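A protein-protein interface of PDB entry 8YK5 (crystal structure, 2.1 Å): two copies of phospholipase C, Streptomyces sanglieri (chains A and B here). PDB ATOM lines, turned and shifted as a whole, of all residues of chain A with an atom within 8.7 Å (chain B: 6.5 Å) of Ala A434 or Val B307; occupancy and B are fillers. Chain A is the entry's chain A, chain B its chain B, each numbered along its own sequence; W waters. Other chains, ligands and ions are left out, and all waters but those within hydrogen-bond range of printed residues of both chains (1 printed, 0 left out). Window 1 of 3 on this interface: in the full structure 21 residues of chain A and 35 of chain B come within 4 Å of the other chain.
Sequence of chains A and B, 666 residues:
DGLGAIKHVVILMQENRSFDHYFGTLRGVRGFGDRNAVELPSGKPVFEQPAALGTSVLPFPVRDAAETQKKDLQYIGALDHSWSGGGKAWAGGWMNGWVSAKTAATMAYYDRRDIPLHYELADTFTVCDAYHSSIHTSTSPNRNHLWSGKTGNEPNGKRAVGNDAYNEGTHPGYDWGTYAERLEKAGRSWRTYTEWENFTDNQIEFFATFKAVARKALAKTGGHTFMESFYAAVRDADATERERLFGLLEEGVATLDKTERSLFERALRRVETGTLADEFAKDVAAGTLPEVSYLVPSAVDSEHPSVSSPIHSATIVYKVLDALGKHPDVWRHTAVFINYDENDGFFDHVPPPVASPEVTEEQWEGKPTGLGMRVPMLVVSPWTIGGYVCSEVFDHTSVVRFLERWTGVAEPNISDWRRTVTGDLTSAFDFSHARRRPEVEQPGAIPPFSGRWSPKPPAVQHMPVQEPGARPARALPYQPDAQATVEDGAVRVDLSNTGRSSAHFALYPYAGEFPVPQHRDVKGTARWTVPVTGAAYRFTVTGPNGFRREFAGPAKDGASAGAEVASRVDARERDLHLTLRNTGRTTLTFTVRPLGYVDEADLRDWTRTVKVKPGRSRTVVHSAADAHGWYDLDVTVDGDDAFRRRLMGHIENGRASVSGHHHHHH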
ATOM      1  N   TRP A 331      -9.184   3.348  17.432  1.00  0.00           N
ATOM      2  CA  TRP A 331      -9.408   3.399  18.868  1.00  0.00           C
ATOM      3  C   TRP A 331      -9.520   4.838  19.373  1.00  0.00           C
ATOM      4  O   TRP A 331     -10.390   5.143  20.202  1.00  0.00           O
ATOM      5  CB  TRP A 331      -8.282   2.666  19.599  1.00  0.00           C
ATOM      6  CG  TRP A 331      -8.533   2.671  21.037  1.00  0.00           C
ATOM      7  CD1 TRP A 331      -9.316   1.808  21.735  1.00  0.00           C
ATOM      8  CD2 TRP A 331      -8.068   3.632  21.968  1.00  0.00           C
ATOM      9  NE1 TRP A 331      -9.350   2.162  23.055  1.00  0.00           N
ATOM     10  CE2 TRP A 331      -8.592   3.287  23.223  1.00  0.00           C
ATOM     11  CE3 TRP A 331      -7.239   4.738  21.869  1.00  0.00           C
ATOM     12  CZ2 TRP A 331      -8.313   4.015  24.366  1.00  0.00           C
ATOM     13  CZ3 TRP A 331      -6.968   5.460  22.999  1.00  0.00           C
ATOM     14  CH2 TRP A 331      -7.499   5.097  24.234  1.00  0.00           C
ATOM     15  N   ARG A 332      -8.683   5.748  18.859  1.00  0.00           N
ATOM     16  CA  ARG A 332      -8.687   7.122  19.374  1.00  0.00           C
ATOM     17  C   ARG A 332      -9.994   7.860  19.113  1.00  0.00           C
ATOM     18  O   ARG A 332     -10.185   8.951  19.651  1.00  0.00           O
ATOM     19  CB  ARG A 332      -7.526   7.943  18.787  1.00  0.00           C
ATOM     20  CG  ARG A 332      -6.176   7.658  19.428  1.00  0.00           C
ATOM     21  CD  ARG A 332      -5.056   8.599  18.943  1.00  0.00           C
ATOM     22  NE  ARG A 332      -4.791   8.516  17.497  1.00  0.00           N
ATOM     23  CZ  ARG A 332      -3.854   7.744  16.945  1.00  0.00           C
ATOM     24  NH1 ARG A 332      -3.084   6.966  17.707  1.00  0.00           N
ATOM     25  NH2 ARG A 332      -3.687   7.753  15.624  1.00  0.00           N
ATOM     26  N   PRO A 382     -11.411   6.473  24.701  1.00  0.00           N
ATOM     27  CA  PRO A 382     -10.271   7.318  25.120  1.00  0.00           C
ATOM     28  C   PRO A 382     -10.659   8.442  26.059  1.00  0.00           C
ATOM     29  O   PRO A 382      -9.766   9.076  26.638  1.00  0.00           O
ATOM     30  CB  PRO A 382      -9.734   7.900  23.804  1.00  0.00           C
ATOM     31  CG  PRO A 382     -10.424   7.191  22.705  1.00  0.00           C
ATOM     32  CD  PRO A 382     -11.675   6.580  23.255  1.00  0.00           C
ATOM     33  N   TRP A 383     -11.953   8.726  26.216  1.00  0.00           N
ATOM     34  CA  TRP A 383     -12.407   9.908  26.935  1.00  0.00           C
ATOM     35  C   TRP A 383     -13.045   9.559  28.265  1.00  0.00           C
ATOM     36  O   TRP A 383     -13.572  10.445  28.941  1.00  0.00           O
ATOM     37  CB  TRP A 383     -13.387  10.709  26.082  1.00  0.00           C
ATOM     38  CG  TRP A 383     -12.924  10.873  24.663  1.00  0.00           C
ATOM     39  CD1 TRP A 383     -11.957  11.728  24.202  1.00  0.00           C
ATOM     40  CD2 TRP A 383     -13.397  10.154  23.523  1.00  0.00           C
ATOM     41  NE1 TRP A 383     -11.807  11.583  22.840  1.00  0.00           N
ATOM     42  CE2 TRP A 383     -12.682  10.626  22.400  1.00  0.00           C
ATOM     43  CE3 TRP A 383     -14.362   9.163  23.339  1.00  0.00           C
ATOM     44  CZ2 TRP A 383     -12.895  10.130  21.123  1.00  0.00           C
ATOM     45  CZ3 TRP A 383     -14.578   8.684  22.075  1.00  0.00           C
ATOM     46  CH2 TRP A 383     -13.857   9.168  20.980  1.00  0.00           C
ATOM     47  N   ILE A 385     -11.342   7.200  30.503  1.00  0.00           N
ATOM     48  CA  ILE A 385     -10.337   6.550  31.341  1.00  0.00           C
ATOM     49  C   ILE A 385     -10.241   7.265  32.687  1.00  0.00           C
ATOM     50  O   ILE A 385     -10.357   8.500  32.770  1.00  0.00           O
ATOM     51  CB  ILE A 385      -8.980   6.527  30.610  1.00  0.00           C
ATOM     52  CG1 ILE A 385      -9.090   5.702  29.327  1.00  0.00           C
ATOM     53  CG2 ILE A 385      -7.848   6.022  31.513  1.00  0.00           C
ATOM     54  CD1 ILE A 385      -8.095   6.106  28.254  1.00  0.00           C
ATOM     55  N   ASP A 430     -15.183  12.815  29.308  1.00  0.00           N
ATOM     56  CA  ASP A 430     -14.337  13.990  29.547  1.00  0.00           C
ATOM     57  C   ASP A 430     -13.440  14.109  28.320  1.00  0.00           C
ATOM     58  O   ASP A 430     -12.480  13.341  28.165  1.00  0.00           O
ATOM     59  CB  ASP A 430     -13.536  13.838  30.839  1.00  0.00           C
ATOM     60  CG  ASP A 430     -12.496  14.960  31.054  1.00  0.00           C
ATOM     61  OD1 ASP A 430     -12.502  15.997  30.346  1.00  0.00           O
ATOM     62  OD2 ASP A 430     -11.669  14.779  31.969  1.00  0.00           O
ATOM     63  N   PHE A 431     -13.767  15.055  27.444  1.00  0.00           N
ATOM     64  CA  PHE A 431     -13.097  15.223  26.157  1.00  0.00           C
ATOM     65  C   PHE A 431     -11.858  16.112  26.212  1.00  0.00           C
ATOM     66  O   PHE A 431     -11.336  16.478  25.156  1.00  0.00           O
ATOM     67  CB  PHE A 431     -14.074  15.806  25.132  1.00  0.00           C
ATOM     68  CG  PHE A 431     -15.170  14.866  24.751  1.00  0.00           C
ATOM     69  CD1 PHE A 431     -14.899  13.766  23.955  1.00  0.00           C
ATOM     70  CD2 PHE A 431     -16.471  15.065  25.203  1.00  0.00           C
ATOM     71  CE1 PHE A 431     -15.902  12.874  23.611  1.00  0.00           C
ATOM     72  CE2 PHE A 431     -17.479  14.192  24.858  1.00  0.00           C
ATOM     73  CZ  PHE A 431     -17.198  13.087  24.059  1.00  0.00           C
ATOM     74  N   SER A 432     -11.356  16.458  27.394  1.00  0.00           N
ATOM     75  CA  SER A 432     -10.356  17.514  27.451  1.00  0.00           C
ATOM     76  C   SER A 432      -8.915  17.023  27.553  1.00  0.00           C
ATOM     77  O   SER A 432      -8.008  17.791  27.214  1.00  0.00           O
ATOM     78  CB  SER A 432     -10.644  18.449  28.628  1.00  0.00           C
ATOM     79  OG  SER A 432     -10.263  17.829  29.848  1.00  0.00           O
ATOM     80  N   HIS A 433      -8.664  15.788  28.010  1.00  0.00           N
ATOM     81  CA  HIS A 433      -7.300  15.301  28.222  1.00  0.00           C
ATOM     82  C   HIS A 433      -7.088  13.952  27.547  1.00  0.00           C
ATOM     83  O   HIS A 433      -7.952  13.074  27.617  1.00  0.00           O
ATOM     84  CB  HIS A 433      -6.964  15.124  29.717  1.00  0.00           C
ATOM     85  CG  HIS A 433      -7.313  16.296  30.571  1.00  0.00           C
ATOM     86  ND1 HIS A 433      -6.709  17.529  30.434  1.00  0.00           N
ATOM     87  CD2 HIS A 433      -8.188  16.420  31.598  1.00  0.00           C
ATOM     88  CE1 HIS A 433      -7.207  18.365  31.331  1.00  0.00           C
ATOM     89  NE2 HIS A 433      -8.107  17.717  32.050  1.00  0.00           N
ATOM     90  N   ALA A 434      -5.923  13.767  26.932  1.00  0.00           N
ATOM     91  CA  ALA A 434      -5.589  12.451  26.406  1.00  0.00           C
ATOM     92  C   ALA A 434      -4.828  11.650  27.455  1.00  0.00           C
ATOM     93  O   ALA A 434      -4.262  12.199  28.400  1.00  0.00           O
ATOM     94  CB  ALA A 434      -4.770  12.565  25.118  1.00  0.00           C
ATOM     95  N   ARG A 435      -4.877  10.330  27.306  1.00  0.00           N
ATOM     96  CA  ARG A 435      -4.164   9.389  28.157  1.00  0.00           C
ATOM     97  C   ARG A 435      -3.649   8.244  27.281  1.00  0.00           C
ATOM     98  O   ARG A 435      -4.018   8.118  26.105  1.00  0.00           O
ATOM     99  CB  ARG A 435      -5.058   8.841  29.292  1.00  0.00           C
ATOM    100  CG  ARG A 435      -5.847   9.815  30.112  1.00  0.00           C
ATOM    101  CD  ARG A 435      -6.033   9.251  31.519  1.00  0.00           C
ATOM    102  NE  ARG A 435      -7.038  10.041  32.198  1.00  0.00           N
ATOM    103  CZ  ARG A 435      -7.274   9.974  33.496  1.00  0.00           C
ATOM    104  NH1 ARG A 435      -6.586   9.145  34.291  1.00  0.00           N
ATOM    105  NH2 ARG A 435      -8.217  10.767  33.975  1.00  0.00           N
ATOM    106  N   ARG A 436      -2.761   7.416  27.834  1.00  0.00           N
ATOM    107  CA  ARG A 436      -2.423   6.205  27.104  1.00  0.00           C
ATOM    108  C   ARG A 436      -3.599   5.228  27.137  1.00  0.00           C
ATOM    109  O   ARG A 436      -4.423   5.228  28.059  1.00  0.00           O
ATOM    110  CB  ARG A 436      -1.154   5.550  27.651  1.00  0.00           C
ATOM    111  CG  ARG A 436      -0.889   5.641  29.125  1.00  0.00           C
ATOM    112  CD  ARG A 436       0.585   5.319  29.339  1.00  0.00           C
ATOM    113  NE  ARG A 436       1.103   5.770  30.625  1.00  0.00           N
ATOM    114  CZ  ARG A 436       2.317   6.264  30.828  1.00  0.00           C
ATOM    115  NH1 ARG A 436       3.189   6.391  29.841  1.00  0.00           N
ATOM    116  NH2 ARG A 436       2.669   6.642  32.031  1.00  0.00           N
ATOM    117  N   ARG A 437      -3.708   4.429  26.097  1.00  0.00           N
ATOM    118  CA  ARG A 437      -4.800   3.482  26.134  1.00  0.00           C
ATOM    119  C   ARG A 437      -4.434   2.340  27.056  1.00  0.00           C
ATOM    120  O   ARG A 437      -3.337   1.785  26.943  1.00  0.00           O
ATOM    121  CB  ARG A 437      -5.181   2.958  24.761  1.00  0.00           C
ATOM    122  CG  ARG A 437      -4.177   2.332  23.934  1.00  0.00           C
ATOM    123  CD  ARG A 437      -4.899   1.645  22.767  1.00  0.00           C
ATOM    124  NE  ARG A 437      -3.884   1.099  21.873  1.00  0.00           N
ATOM    125  CZ  ARG A 437      -3.527  -0.180  21.833  1.00  0.00           C
ATOM    126  NH1 ARG A 437      -4.136  -1.074  22.613  1.00  0.00           N
ATOM    127  NH2 ARG A 437      -2.563  -0.560  21.000  1.00  0.00           N
ATOM    128  N   TYR B  75       3.013  15.398  15.909  1.00  0.00           N
ATOM    129  CA  TYR B  75       1.906  14.824  16.662  1.00  0.00           C
ATOM    130  C   TYR B  75       1.479  13.441  16.162  1.00  0.00           C
ATOM    131  O   TYR B  75       0.295  13.106  16.196  1.00  0.00           O
ATOM    132  CB  TYR B  75       0.738  15.810  16.650  1.00  0.00           C
ATOM    133  CG  TYR B  75       1.088  17.128  17.347  1.00  0.00           C
ATOM    134  CD1 TYR B  75       1.546  17.135  18.655  1.00  0.00           C
ATOM    135  CD2 TYR B  75       0.963  18.350  16.698  1.00  0.00           C
ATOM    136  CE1 TYR B  75       1.860  18.315  19.312  1.00  0.00           C
ATOM    137  CE2 TYR B  75       1.274  19.561  17.350  1.00  0.00           C
ATOM    138  CZ  TYR B  75       1.719  19.523  18.659  1.00  0.00           C
ATOM    139  OH  TYR B  75       2.043  20.677  19.325  1.00  0.00           O
ATOM    140  N   PHE B 199       1.706  12.097  34.782  1.00  0.00           N
ATOM    141  CA  PHE B 199       1.489  11.080  33.761  1.00  0.00           C
ATOM    142  C   PHE B 199       1.824   9.691  34.274  1.00  0.00           C
ATOM    143  O   PHE B 199       2.349   8.862  33.531  1.00  0.00           O
ATOM    144  CB  PHE B 199       2.317  11.389  32.513  1.00  0.00           C
ATOM    145  CG  PHE B 199       1.854  10.684  31.277  1.00  0.00           C
ATOM    146  CD1 PHE B 199       2.776  10.124  30.403  1.00  0.00           C
ATOM    147  CD2 PHE B 199       0.509  10.602  30.966  1.00  0.00           C
ATOM    148  CE1 PHE B 199       2.358   9.489  29.257  1.00  0.00           C
ATOM    149  CE2 PHE B 199       0.096   9.967  29.813  1.00  0.00           C
ATOM    150  CZ  PHE B 199       1.024   9.414  28.964  1.00  0.00           C
ATOM    151  N   SER B 298       5.718  16.419  33.104  1.00  0.00           N
ATOM    152  CA  SER B 298       4.294  16.222  32.911  1.00  0.00           C
ATOM    153  C   SER B 298       4.026  15.418  31.640  1.00  0.00           C
ATOM    154  O   SER B 298       4.923  15.155  30.831  1.00  0.00           O
ATOM    155  CB  SER B 298       3.590  17.568  32.828  1.00  0.00           C
ATOM    156  OG  SER B 298       3.919  18.161  31.585  1.00  0.00           O
ATOM    157  N   ALA B 299       2.755  15.035  31.471  1.00  0.00           N
ATOM    158  CA  ALA B 299       2.345  14.312  30.271  1.00  0.00           C
ATOM    159  C   ALA B 299       2.705  15.089  29.017  1.00  0.00           C
ATOM    160  O   ALA B 299       3.351  14.555  28.108  1.00  0.00           O
ATOM    161  CB  ALA B 299       0.842  14.017  30.307  1.00  0.00           C
ATOM    162  N   VAL B 300       2.305  16.362  28.950  1.00  0.00           N
ATOM    163  CA  VAL B 300       2.567  17.154  27.760  1.00  0.00           C
ATOM    164  C   VAL B 300       4.069  17.363  27.510  1.00  0.00           C
ATOM    165  O   VAL B 300       4.465  17.642  26.374  1.00  0.00           O
ATOM    166  CB  VAL B 300       1.806  18.503  27.859  1.00  0.00           C
ATOM    167  CG1 VAL B 300       2.458  19.435  28.859  1.00  0.00           C
ATOM    168  CG2 VAL B 300       1.709  19.169  26.499  1.00  0.00           C
ATOM    169  N   ASP B 301       4.921  17.217  28.529  1.00  0.00           N
ATOM    170  CA  ASP B 301       6.361  17.424  28.360  1.00  0.00           C
ATOM    171  C   ASP B 301       7.157  16.126  28.245  1.00  0.00           C
ATOM    172  O   ASP B 301       8.374  16.193  28.068  1.00  0.00           O
ATOM    173  CB  ASP B 301       6.947  18.237  29.521  1.00  0.00           C
ATOM    174  CG  ASP B 301       6.478  19.688  29.539  1.00  0.00           C
ATOM    175  OD1 ASP B 301       6.119  20.247  28.464  1.00  0.00           O
ATOM    176  OD2 ASP B 301       6.475  20.263  30.659  1.00  0.00           O
ATOM    177  N   SER B 302       6.500  14.954  28.300  1.00  0.00           N
ATOM    178  CA  SER B 302       7.173  13.664  28.457  1.00  0.00           C
ATOM    179  C   SER B 302       7.722  13.073  27.164  1.00  0.00           C
ATOM    180  O   SER B 302       8.442  12.075  27.237  1.00  0.00           O
ATOM    181  CB  SER B 302       6.211  12.641  29.068  1.00  0.00           C
ATOM    182  OG  SER B 302       5.142  12.376  28.179  1.00  0.00           O
ATOM    183  N   GLU B 303       7.390  13.645  26.009  1.00  0.00           N
ATOM    184  CA  GLU B 303       7.665  13.097  24.682  1.00  0.00           C
ATOM    185  C   GLU B 303       6.782  11.902  24.317  1.00  0.00           C
ATOM    186  O   GLU B 303       6.858  11.419  23.184  1.00  0.00           O
ATOM    187  CB  GLU B 303       9.149  12.707  24.522  1.00  0.00           C
ATOM    188  CG  GLU B 303       9.660  12.933  23.108  1.00  0.00           C
ATOM    189  CD  GLU B 303      11.164  13.209  23.036  1.00  0.00           C
ATOM    190  OE1 GLU B 303      11.642  13.545  21.940  1.00  0.00           O
ATOM    191  OE2 GLU B 303      11.868  13.105  24.061  1.00  0.00           O
ATOM    192  N   HIS B 304       5.934  11.432  25.227  1.00  0.00           N
ATOM    193  CA  HIS B 304       5.069  10.290  24.914  1.00  0.00           C
ATOM    194  C   HIS B 304       4.151  10.603  23.727  1.00  0.00           C
ATOM    195  O   HIS B 304       3.463  11.632  23.738  1.00  0.00           O
ATOM    196  CB  HIS B 304       4.221   9.899  26.118  1.00  0.00           C
ATOM    197  CG  HIS B 304       3.524   8.591  25.940  1.00  0.00           C
ATOM    198  ND1 HIS B 304       2.472   8.423  25.062  1.00  0.00           N
ATOM    199  CD2 HIS B 304       3.749   7.378  26.497  1.00  0.00           C
ATOM    200  CE1 HIS B 304       2.075   7.164  25.091  1.00  0.00           C
ATOM    201  NE2 HIS B 304       2.834   6.512  25.951  1.00  0.00           N
ATOM    202  N   PRO B 305       4.099   9.747  22.697  1.00  0.00           N
ATOM    203  CA  PRO B 305       3.337  10.108  21.485  1.00  0.00           C
ATOM    204  C   PRO B 305       1.826  10.236  21.687  1.00  0.00           C
ATOM    205  O   PRO B 305       1.147  10.746  20.786  1.00  0.00           O
ATOM    206  CB  PRO B 305       3.665   8.989  20.490  1.00  0.00           C
ATOM    207  CG  PRO B 305       4.476   7.967  21.248  1.00  0.00           C
ATOM    208  CD  PRO B 305       4.988   8.589  22.494  1.00  0.00           C
ATOM    209  N   SER B 306       1.258   9.833  22.811  1.00  0.00           N
ATOM    210  CA  SER B 306      -0.175  10.071  22.918  1.00  0.00           C
ATOM    211  C   SER B 306      -0.513  11.372  23.644  1.00  0.00           C
ATOM    212  O   SER B 306      -1.686  11.772  23.636  1.00  0.00           O
ATOM    213  CB  SER B 306      -0.884   8.862  23.561  1.00  0.00           C
ATOM    214  OG  SER B 306      -0.552   8.708  24.918  1.00  0.00           O
ATOM    215  N   VAL B 307       0.485  12.093  24.183  1.00  0.00           N
ATOM    216  CA  VAL B 307       0.212  13.296  24.962  1.00  0.00           C
ATOM    217  C   VAL B 307       1.195  14.423  24.672  1.00  0.00           C
ATOM    218  O   VAL B 307       0.958  15.557  25.089  1.00  0.00           O
ATOM    219  CB  VAL B 307       0.212  13.008  26.476  1.00  0.00           C
ATOM    220  CG1 VAL B 307      -1.068  12.248  26.905  1.00  0.00           C
ATOM    221  CG2 VAL B 307       1.508  12.283  26.906  1.00  0.00           C
ATOM    222  N   SER B 308       2.295  14.138  23.968  1.00  0.00           N
ATOM    223  CA  SER B 308       3.398  15.098  23.881  1.00  0.00           C
ATOM    224  C   SER B 308       3.926  15.199  22.450  1.00  0.00           C
ATOM    225  O   SER B 308       3.153  15.044  21.500  1.00  0.00           O
ATOM    226  CB  SER B 308       4.495  14.692  24.877  1.00  0.00           C
ATOM    227  OG  SER B 308       5.607  15.585  24.884  1.00  0.00           O
ATOM    228  N   SER B 309       5.218  15.470  22.284  1.00  0.00           N
ATOM    229  CA  SER B 309       5.858  15.608  20.978  1.00  0.00           C
ATOM    230  C   SER B 309       7.375  15.718  21.188  1.00  0.00           C
ATOM    231  O   SER B 309       7.833  16.002  22.305  1.00  0.00           O
ATOM    232  CB  SER B 309       5.360  16.847  20.222  1.00  0.00           C
ATOM    233  OG  SER B 309       5.926  18.032  20.796  1.00  0.00           O
ATOM    234  N   HIS B 312       8.030  19.356  22.282  1.00  0.00           N
ATOM    235  CA  HIS B 312       7.691  19.572  23.687  1.00  0.00           C
ATOM    236  C   HIS B 312       8.804  19.076  24.584  1.00  0.00           C
ATOM    237  O   HIS B 312       9.118  19.692  25.609  1.00  0.00           O
ATOM    238  CB  HIS B 312       6.395  18.857  24.056  1.00  0.00           C
ATOM    239  CG  HIS B 312       5.153  19.628  23.738  1.00  0.00           C
ATOM    240  ND1 HIS B 312       4.429  19.432  22.580  1.00  0.00           N
ATOM    241  CD2 HIS B 312       4.490  20.577  24.442  1.00  0.00           C
ATOM    242  CE1 HIS B 312       3.372  20.227  22.585  1.00  0.00           C
ATOM    243  NE2 HIS B 312       3.388  20.935  23.701  1.00  0.00           N
ATOM    244  N   ARG B 452      -3.804  13.770  16.795  1.00  0.00           N
ATOM    245  CA  ARG B 452      -2.987  12.581  16.599  1.00  0.00           C
ATOM    246  C   ARG B 452      -3.325  11.886  15.279  1.00  0.00           C
ATOM    247  O   ARG B 452      -4.452  11.950  14.789  1.00  0.00           O
ATOM    248  CB  ARG B 452      -3.189  11.600  17.750  1.00  0.00           C
ATOM    249  CG  ARG B 452      -2.820  12.156  19.094  1.00  0.00           C
ATOM    250  CD  ARG B 452      -1.308  12.410  19.196  1.00  0.00           C
ATOM    251  NE  ARG B 452      -1.046  13.437  20.198  1.00  0.00           N
ATOM    252  CZ  ARG B 452       0.163  13.898  20.515  1.00  0.00           C
ATOM    253  NH1 ARG B 452       1.257  13.420  19.904  1.00  0.00           N
ATOM    254  NH2 ARG B 452       0.285  14.835  21.453  1.00  0.00           N
HETATM  255  O   HOH W   1      -5.773   8.917  14.727  1.00  0.00           O
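Water W1 bridges NH2 of Arg A332 and O of Arg B452.
Among the printed residues, pairs that only touch across the chains: Arg A332 with Arg B452 (3.5 Å), Ala A434 with Ser B306 (3.5 Å), Ala A434 with Val B307 (3.5 Å), Arg A435 with Ser B306 (3.7 Å), Arg A436 with His B304 (3.5 Å) and Arg A436 with Ser B306 (3.8 Å).
Of the printed residues of chain B, Ala A434 touches Ser B306 and Val B307.
Ser B306 touches just these residues of chain A: Ala A434 (3.5 Å), Arg A435 (3.7 Å) and Arg A436 (3.8 Å).
Printed residues of chain A within 4 Å of Phe B199: Arg A436.
Printed residues of chain A within 4 Å of His B304: Arg A436 (3.5 Å).
Of the printed residues of chain B, Arg A332 touches Arg B452.
Asp A430 touches none of the printed residues of chain B.
The nearest residue of chain A that does not touch Val B307 is Arg A435 (4.3 Å).
The nearest printed residue of chain B that does not touch Arg A436 is Val B307 (5.2 Å).
Of the 13 printed residues of chain A, 4 touch a printed residue of chain B.
Among the printed residues, 7 pairs touch across the chains.
No position is printed for both chains.
Of the 7 pairs that touch across the chains among the printed residues, none has its exchanged pair printed and touching as well.
The guanidinium group (NH2) of Arg A436 lies within hydrogen-bond range of the backbone carbonyl oxygen (O) of Phe B199 (2.7 Å).
The backbone carbonyl oxygen (O) of Ile A385 lies within hydrogen-bond range of the guanidinium group (NH2) of Arg A435.
N of His B304 sits close to OG of Ser B302 (3.2 Å).
N of Ser B306 sits at hydrogen-bond distance from ND1 of His B304.
The backbone carbonyl oxygen of Pro B305 sits at hydrogen-bond distance from the guanidinium group of Arg B452.
The guanidinium group of Arg B452 sits at hydrogen-bond distance from the backbone carbonyl oxygen of Ser B308 (2.9 Å).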
